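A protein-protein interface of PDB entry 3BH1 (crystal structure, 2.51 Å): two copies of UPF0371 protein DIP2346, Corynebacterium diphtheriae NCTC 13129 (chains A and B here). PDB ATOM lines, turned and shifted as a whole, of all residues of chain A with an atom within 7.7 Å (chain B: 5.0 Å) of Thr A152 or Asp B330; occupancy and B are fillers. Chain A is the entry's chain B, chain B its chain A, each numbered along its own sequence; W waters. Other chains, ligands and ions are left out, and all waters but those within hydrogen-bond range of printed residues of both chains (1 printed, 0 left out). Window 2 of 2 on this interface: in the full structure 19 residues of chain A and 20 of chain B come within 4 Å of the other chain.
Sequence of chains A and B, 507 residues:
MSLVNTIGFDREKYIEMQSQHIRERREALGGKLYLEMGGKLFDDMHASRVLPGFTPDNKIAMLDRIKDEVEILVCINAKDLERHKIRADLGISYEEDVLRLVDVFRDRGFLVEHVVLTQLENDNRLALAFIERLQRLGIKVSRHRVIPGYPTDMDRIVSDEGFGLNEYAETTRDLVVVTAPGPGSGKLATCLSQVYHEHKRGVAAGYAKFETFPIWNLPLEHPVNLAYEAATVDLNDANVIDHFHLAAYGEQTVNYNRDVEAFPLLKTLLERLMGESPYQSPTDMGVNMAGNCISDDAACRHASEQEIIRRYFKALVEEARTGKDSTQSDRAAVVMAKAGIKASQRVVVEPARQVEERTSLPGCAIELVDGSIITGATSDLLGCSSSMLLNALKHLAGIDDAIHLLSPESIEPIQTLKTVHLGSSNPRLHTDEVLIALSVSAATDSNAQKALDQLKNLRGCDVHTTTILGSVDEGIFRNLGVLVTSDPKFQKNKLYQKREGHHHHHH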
ATOM      1  N   PRO A 148       6.429   0.533   1.849  1.00  0.00           N
ATOM      2  CA  PRO A 148       7.408   1.575   1.526  1.00  0.00           C
ATOM      3  C   PRO A 148       8.207   1.246   0.267  1.00  0.00           C
ATOM      4  O   PRO A 148       8.709   0.129   0.128  1.00  0.00           O
ATOM      5  CB  PRO A 148       8.333   1.588   2.755  1.00  0.00           C
ATOM      6  CG  PRO A 148       7.562   0.923   3.837  1.00  0.00           C
ATOM      7  CD  PRO A 148       6.724  -0.102   3.146  1.00  0.00           C
ATOM      8  N   GLY A 149       8.290   2.212  -0.646  1.00  0.00           N
ATOM      9  CA  GLY A 149       9.044   2.056  -1.885  1.00  0.00           C
ATOM     10  C   GLY A 149       8.417   1.137  -2.917  1.00  0.00           C
ATOM     11  O   GLY A 149       9.113   0.610  -3.779  1.00  0.00           O
ATOM     12  N   TYR A 150       7.106   0.934  -2.830  1.00  0.00           N
ATOM     13  CA  TYR A 150       6.371   0.191  -3.852  1.00  0.00           C
ATOM     14  C   TYR A 150       6.001   1.157  -4.982  1.00  0.00           C
ATOM     15  O   TYR A 150       5.576   2.282  -4.704  1.00  0.00           O
ATOM     16  CB  TYR A 150       5.116  -0.461  -3.243  1.00  0.00           C
ATOM     17  CG  TYR A 150       4.358  -1.395  -4.175  1.00  0.00           C
ATOM     18  CD1 TYR A 150       4.755  -2.722  -4.335  1.00  0.00           C
ATOM     19  CD2 TYR A 150       3.241  -0.954  -4.889  1.00  0.00           C
ATOM     20  CE1 TYR A 150       4.072  -3.582  -5.193  1.00  0.00           C
ATOM     21  CE2 TYR A 150       2.546  -1.808  -5.745  1.00  0.00           C
ATOM     22  CZ  TYR A 150       2.969  -3.121  -5.891  1.00  0.00           C
ATOM     23  OH  TYR A 150       2.293  -3.976  -6.733  1.00  0.00           O
ATOM     24  N   PRO A 151       6.150   0.733  -6.260  1.00  0.00           N
ATOM     25  CA  PRO A 151       6.665  -0.539  -6.766  1.00  0.00           C
ATOM     26  C   PRO A 151       8.117  -0.526  -7.268  1.00  0.00           C
ATOM     27  O   PRO A 151       8.490  -1.390  -8.070  1.00  0.00           O
ATOM     28  CB  PRO A 151       5.737  -0.807  -7.951  1.00  0.00           C
ATOM     29  CG  PRO A 151       5.438   0.581  -8.497  1.00  0.00           C
ATOM     30  CD  PRO A 151       5.678   1.579  -7.373  1.00  0.00           C
ATOM     31  N   THR A 152       8.930   0.420  -6.805  1.00  0.00           N
ATOM     32  CA  THR A 152      10.281   0.585  -7.363  1.00  0.00           C
ATOM     33  C   THR A 152      11.409  -0.007  -6.520  1.00  0.00           C
ATOM     34  O   THR A 152      12.336  -0.603  -7.072  1.00  0.00           O
ATOM     35  CB  THR A 152      10.590   2.062  -7.708  1.00  0.00           C
ATOM     36  OG1 THR A 152      10.645   2.843  -6.507  1.00  0.00           O
ATOM     37  CG2 THR A 152       9.518   2.629  -8.627  1.00  0.00           C
ATOM     38  N   ASP A 153      11.323   0.142  -5.196  1.00  0.00           N
ATOM     39  CA  ASP A 153      12.386  -0.298  -4.282  1.00  0.00           C
ATOM     40  C   ASP A 153      12.364  -1.815  -4.046  1.00  0.00           C
ATOM     41  O   ASP A 153      11.876  -2.305  -3.024  1.00  0.00           O
ATOM     42  CB  ASP A 153      12.313   0.474  -2.957  1.00  0.00           C
ATOM     43  CG  ASP A 153      13.650   0.533  -2.227  1.00  0.00           C
ATOM     44  OD1 ASP A 153      13.793   1.402  -1.340  1.00  0.00           O
ATOM     45  OD2 ASP A 153      14.556  -0.276  -2.530  1.00  0.00           O
ATOM     46  N   MET A 154      12.942  -2.536  -5.000  1.00  0.00           N
ATOM     47  CA  MET A 154      12.929  -3.996  -5.042  1.00  0.00           C
ATOM     48  C   MET A 154      13.501  -4.699  -3.810  1.00  0.00           C
ATOM     49  O   MET A 154      12.933  -5.691  -3.347  1.00  0.00           O
ATOM     50  CB  MET A 154      13.648  -4.477  -6.310  1.00  0.00           C
ATOM     51  CG  MET A 154      12.994  -4.012  -7.619  1.00  0.00           C
ATOM     52  SD  MET A 154      11.363  -4.748  -7.904  1.00  0.00           S
ATOM     53  CE  MET A 154      11.728  -6.408  -7.370  1.00  0.00           C
ATOM     54  N   ASP A 155      14.613  -4.177  -3.288  1.00  0.00           N
ATOM     55  CA  ASP A 155      15.226  -4.684  -2.055  1.00  0.00           C
ATOM     56  C   ASP A 155      14.289  -4.539  -0.857  1.00  0.00           C
ATOM     57  O   ASP A 155      14.144  -5.475  -0.068  1.00  0.00           O
ATOM     58  CB  ASP A 155      16.549  -3.967  -1.757  1.00  0.00           C
ATOM     59  CG  ASP A 155      17.708  -4.479  -2.600  1.00  0.00           C
ATOM     60  OD1 ASP A 155      17.667  -5.636  -3.060  1.00  0.00           O
ATOM     61  OD2 ASP A 155      18.678  -3.719  -2.791  1.00  0.00           O
ATOM     62  N   ARG A 156      13.658  -3.372  -0.735  1.00  0.00           N
ATOM     63  CA  ARG A 156      12.729  -3.093   0.359  1.00  0.00           C
ATOM     64  C   ARG A 156      11.416  -3.879   0.254  1.00  0.00           C
ATOM     65  O   ARG A 156      10.911  -4.368   1.263  1.00  0.00           O
ATOM     66  CB  ARG A 156      12.461  -1.586   0.481  1.00  0.00           C
ATOM     67  CG  ARG A 156      11.460  -1.214   1.565  1.00  0.00           C
ATOM     68  CD  ARG A 156      11.864   0.039   2.308  1.00  0.00           C
ATOM     69  NE  ARG A 156      12.960  -0.218   3.238  1.00  0.00           N
ATOM     70  CZ  ARG A 156      13.241   0.537   4.293  1.00  0.00           C
ATOM     71  NH1 ARG A 156      12.501   1.605   4.570  1.00  0.00           N
ATOM     72  NH2 ARG A 156      14.258   0.219   5.081  1.00  0.00           N
ATOM     73  N   ILE A 157      10.878  -4.007  -0.961  1.00  0.00           N
ATOM     74  CA  ILE A 157       9.602  -4.701  -1.173  1.00  0.00           C
ATOM     75  C   ILE A 157       9.697  -6.183  -0.785  1.00  0.00           C
ATOM     76  O   ILE A 157       8.995  -6.627   0.130  1.00  0.00           O
ATOM     77  CB  ILE A 157       9.072  -4.525  -2.620  1.00  0.00           C
ATOM     78  CG1 ILE A 157       8.728  -3.061  -2.894  1.00  0.00           C
ATOM     79  CG2 ILE A 157       7.815  -5.354  -2.850  1.00  0.00           C
ATOM     80  CD1 ILE A 157       8.650  -2.732  -4.362  1.00  0.00           C
ATOM     81  N   GLU A 261       2.552  -0.657 -19.453  1.00  0.00           N
ATOM     82  CA  GLU A 261       3.308   0.331 -18.685  1.00  0.00           C
ATOM     83  C   GLU A 261       3.798  -0.209 -17.325  1.00  0.00           C
ATOM     84  O   GLU A 261       4.859   0.184 -16.855  1.00  0.00           O
ATOM     85  CB  GLU A 261       2.473   1.613 -18.548  1.00  0.00           C
ATOM     86  CG  GLU A 261       2.358   2.232 -17.154  1.00  0.00           C
ATOM     87  CD  GLU A 261       3.236   3.455 -16.976  1.00  0.00           C
ATOM     88  OE1 GLU A 261       2.977   4.484 -17.645  1.00  0.00           O
ATOM     89  OE2 GLU A 261       4.172   3.393 -16.153  1.00  0.00           O
ATOM     90  N   LEU A 265       8.249  -3.375 -14.016  1.00  0.00           N
ATOM     91  CA  LEU A 265       8.439  -3.456 -12.566  1.00  0.00           C
ATOM     92  C   LEU A 265       7.860  -4.732 -11.962  1.00  0.00           C
ATOM     93  O   LEU A 265       8.363  -5.227 -10.948  1.00  0.00           O
ATOM     94  CB  LEU A 265       7.902  -2.218 -11.848  1.00  0.00           C
ATOM     95  CG  LEU A 265       8.707  -0.940 -12.099  1.00  0.00           C
ATOM     96  CD1 LEU A 265       8.149   0.222 -11.298  1.00  0.00           C
ATOM     97  CD2 LEU A 265      10.186  -1.147 -11.780  1.00  0.00           C
ATOM     98  N   THR A 268      10.495  -7.633 -12.737  1.00  0.00           N
ATOM     99  CA  THR A 268      11.567  -7.555 -11.747  1.00  0.00           C
ATOM    100  C   THR A 268      11.094  -8.109 -10.405  1.00  0.00           C
ATOM    101  O   THR A 268      11.815  -8.862  -9.753  1.00  0.00           O
ATOM    102  CB  THR A 268      12.038  -6.106 -11.550  1.00  0.00           C
ATOM    103  OG1 THR A 268      12.151  -5.464 -12.825  1.00  0.00           O
ATOM    104  CG2 THR A 268      13.385  -6.071 -10.841  1.00  0.00           C
ATOM    105  N   LEU A 269       9.874  -7.738 -10.016  1.00  0.00           N
ATOM    106  CA  LEU A 269       9.275  -8.193  -8.768  1.00  0.00           C
ATOM    107  C   LEU A 269       9.101  -9.708  -8.725  1.00  0.00           C
ATOM    108  O   LEU A 269       9.427 -10.341  -7.723  1.00  0.00           O
ATOM    109  CB  LEU A 269       7.958  -7.460  -8.513  1.00  0.00           C
ATOM    110  CG  LEU A 269       7.382  -7.317  -7.102  1.00  0.00           C
ATOM    111  CD1 LEU A 269       8.424  -7.429  -6.028  1.00  0.00           C
ATOM    112  CD2 LEU A 269       6.653  -5.986  -6.980  1.00  0.00           C
ATOM    113  N   SER B 326       4.488  10.293  -6.452  1.00  0.00           N
ATOM    114  CA  SER B 326       5.631   9.750  -7.176  1.00  0.00           C
ATOM    115  C   SER B 326       5.329   9.181  -8.563  1.00  0.00           C
ATOM    116  O   SER B 326       6.153   8.449  -9.111  1.00  0.00           O
ATOM    117  CB  SER B 326       6.346   8.690  -6.320  1.00  0.00           C
ATOM    118  OG  SER B 326       5.661   7.450  -6.366  1.00  0.00           O
ATOM    119  N   THR B 327       4.177   9.539  -9.133  1.00  0.00           N
ATOM    120  CA  THR B 327       3.774   9.087 -10.479  1.00  0.00           C
ATOM    121  C   THR B 327       4.886   9.212 -11.536  1.00  0.00           C
ATOM    122  O   THR B 327       5.185   8.240 -12.250  1.00  0.00           O
ATOM    123  CB  THR B 327       2.498   9.831 -10.965  1.00  0.00           C
ATOM    124  OG1 THR B 327       1.440   9.615 -10.028  1.00  0.00           O
ATOM    125  CG2 THR B 327       2.044   9.351 -12.352  1.00  0.00           C
ATOM    126  N   GLN B 328       5.520  10.383 -11.595  1.00  0.00           N
ATOM    127  CA  GLN B 328       6.509  10.690 -12.629  1.00  0.00           C
ATOM    128  C   GLN B 328       7.841   9.976 -12.405  1.00  0.00           C
ATOM    129  O   GLN B 328       8.457   9.481 -13.356  1.00  0.00           O
ATOM    130  CB  GLN B 328       6.743  12.203 -12.745  1.00  0.00           C
ATOM    131  CG  GLN B 328       5.489  13.080 -12.707  1.00  0.00           C
ATOM    132  CD  GLN B 328       5.272  13.746 -11.351  1.00  0.00           C
ATOM    133  OE1 GLN B 328       5.659  14.901 -11.147  1.00  0.00           O
ATOM    134  NE2 GLN B 328       4.662  13.020 -10.416  1.00  0.00           N
ATOM    135  N   SER B 329       8.289   9.931 -11.147  1.00  0.00           N
ATOM    136  CA  SER B 329       9.563   9.278 -10.829  1.00  0.00           C
ATOM    137  C   SER B 329       9.446   7.765 -10.963  1.00  0.00           C
ATOM    138  O   SER B 329      10.382   7.108 -11.439  1.00  0.00           O
ATOM    139  CB  SER B 329      10.096   9.675  -9.452  1.00  0.00           C
ATOM    140  OG  SER B 329       9.202   9.308  -8.415  1.00  0.00           O
ATOM    141  N   ASP B 330       8.291   7.226 -10.567  1.00  0.00           N
ATOM    142  CA  ASP B 330       7.963   5.821 -10.823  1.00  0.00           C
ATOM    143  C   ASP B 330       7.971   5.494 -12.318  1.00  0.00           C
ATOM    144  O   ASP B 330       8.551   4.485 -12.724  1.00  0.00           O
ATOM    145  CB  ASP B 330       6.622   5.445 -10.199  1.00  0.00           C
ATOM    146  CG  ASP B 330       6.671   5.413  -8.676  1.00  0.00           C
ATOM    147  OD1 ASP B 330       7.770   5.544  -8.090  1.00  0.00           O
ATOM    148  OD2 ASP B 330       5.600   5.258  -8.060  1.00  0.00           O
ATOM    149  N   ARG B 331       7.359   6.362 -13.128  1.00  0.00           N
ATOM    150  CA  ARG B 331       7.389   6.221 -14.593  1.00  0.00           C
ATOM    151  C   ARG B 331       8.810   6.172 -15.166  1.00  0.00           C
ATOM    152  O   ARG B 331       9.081   5.376 -16.061  1.00  0.00           O
ATOM    153  CB  ARG B 331       6.554   7.312 -15.288  1.00  0.00           C
ATOM    154  CG  ARG B 331       5.072   6.946 -15.485  1.00  0.00           C
ATOM    155  CD  ARG B 331       4.256   8.054 -16.174  1.00  0.00           C
ATOM    156  NE  ARG B 331       4.466   8.117 -17.626  1.00  0.00           N
ATOM    157  CZ  ARG B 331       5.180   9.050 -18.262  1.00  0.00           C
ATOM    158  NH1 ARG B 331       5.772  10.029 -17.590  1.00  0.00           N
ATOM    159  NH2 ARG B 331       5.303   9.009 -19.584  1.00  0.00           N
ATOM    160  N   ALA B 332       9.718   6.997 -14.636  1.00  0.00           N
ATOM    161  CA  ALA B 332      11.127   6.968 -15.063  1.00  0.00           C
ATOM    162  C   ALA B 332      11.860   5.697 -14.618  1.00  0.00           C
ATOM    163  O   ALA B 332      12.728   5.206 -15.340  1.00  0.00           O
ATOM    164  CB  ALA B 332      11.868   8.205 -14.591  1.00  0.00           C
ATOM    165  N   ALA B 333      11.504   5.170 -13.444  1.00  0.00           N
ATOM    166  CA  ALA B 333      12.062   3.903 -12.955  1.00  0.00           C
ATOM    167  C   ALA B 333      11.703   2.720 -13.857  1.00  0.00           C
ATOM    168  O   ALA B 333      12.522   1.817 -14.054  1.00  0.00           O
ATOM    169  CB  ALA B 333      11.613   3.633 -11.526  1.00  0.00           C
ATOM    170  N   VAL B 334      10.477   2.738 -14.388  1.00  0.00           N
ATOM    171  CA  VAL B 334       9.994   1.755 -15.363  1.00  0.00           C
ATOM    172  C   VAL B 334      10.909   1.770 -16.589  1.00  0.00           C
ATOM    173  O   VAL B 334      11.356   0.718 -17.069  1.00  0.00           O
ATOM    174  CB  VAL B 334       8.525   2.055 -15.799  1.00  0.00           C
ATOM    175  CG1 VAL B 334       8.083   1.143 -16.937  1.00  0.00           C
ATOM    176  CG2 VAL B 334       7.556   1.937 -14.621  1.00  0.00           C
HETATM  177  O   HOH W   1       8.366   3.792  -5.721  1.00  0.00           O
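The side-chain carboxylate of Glu A261 lies within salt-bridge range of the guanidinium group of Arg B331.
The side-chain hydroxyl (OG) of Ser B326 lies within hydrogen-bond range of the side-chain carboxylate (OD2) of Asp B330 (2.8 Å).
Among the printed residues, pairs that only touch across the chains: Pro A151 with Asp B330, Thr A152 with Asp B330, Thr A152 with Ala B333, Glu A261 with Val B334 and Leu A265 with Val B334.
Thr A152 touches just these residues of chain B: Asp B330 and Ala B333. Of chain A, only Pro A151 (3.7 Å) and Thr A152 (3.4 Å) come within 4 Å of Asp B330. Printed residues of chain A within 4 Å of Val B334: Glu A261 (3.4 Å) and Leu A265 (3.8 Å). Printed residues of chain B within 4 Å of Glu A261: Arg B331 (3.7 Å) and Val B334 (3.4 Å). Of the printed residues of chain B, Pro A151 touches Asp B330. Of the printed residues of chain B, Leu A265 touches Val B334. Printed residues of chain A within 4 Å of Ala B333: Thr A152 (3.7 Å). Thr A268 touches none of the printed residues of chain B.
Of the 9 printed residues of chain B, 4 touch a printed residue of chain A. Hydrophobic or aromatic side chains of chain B within 4 Å of the printed part of chain A: Ala B333 and Val B334. Among the printed residues, 6 pairs touch across the chains.
No position is printed for both chains.
Water W1 lies within hydrogen-bond range of OG1 of Thr A152 (2.6 Å), OD1 of Asp B330 (3.0 Å) and O of Tyr A150 (3.3 Å).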
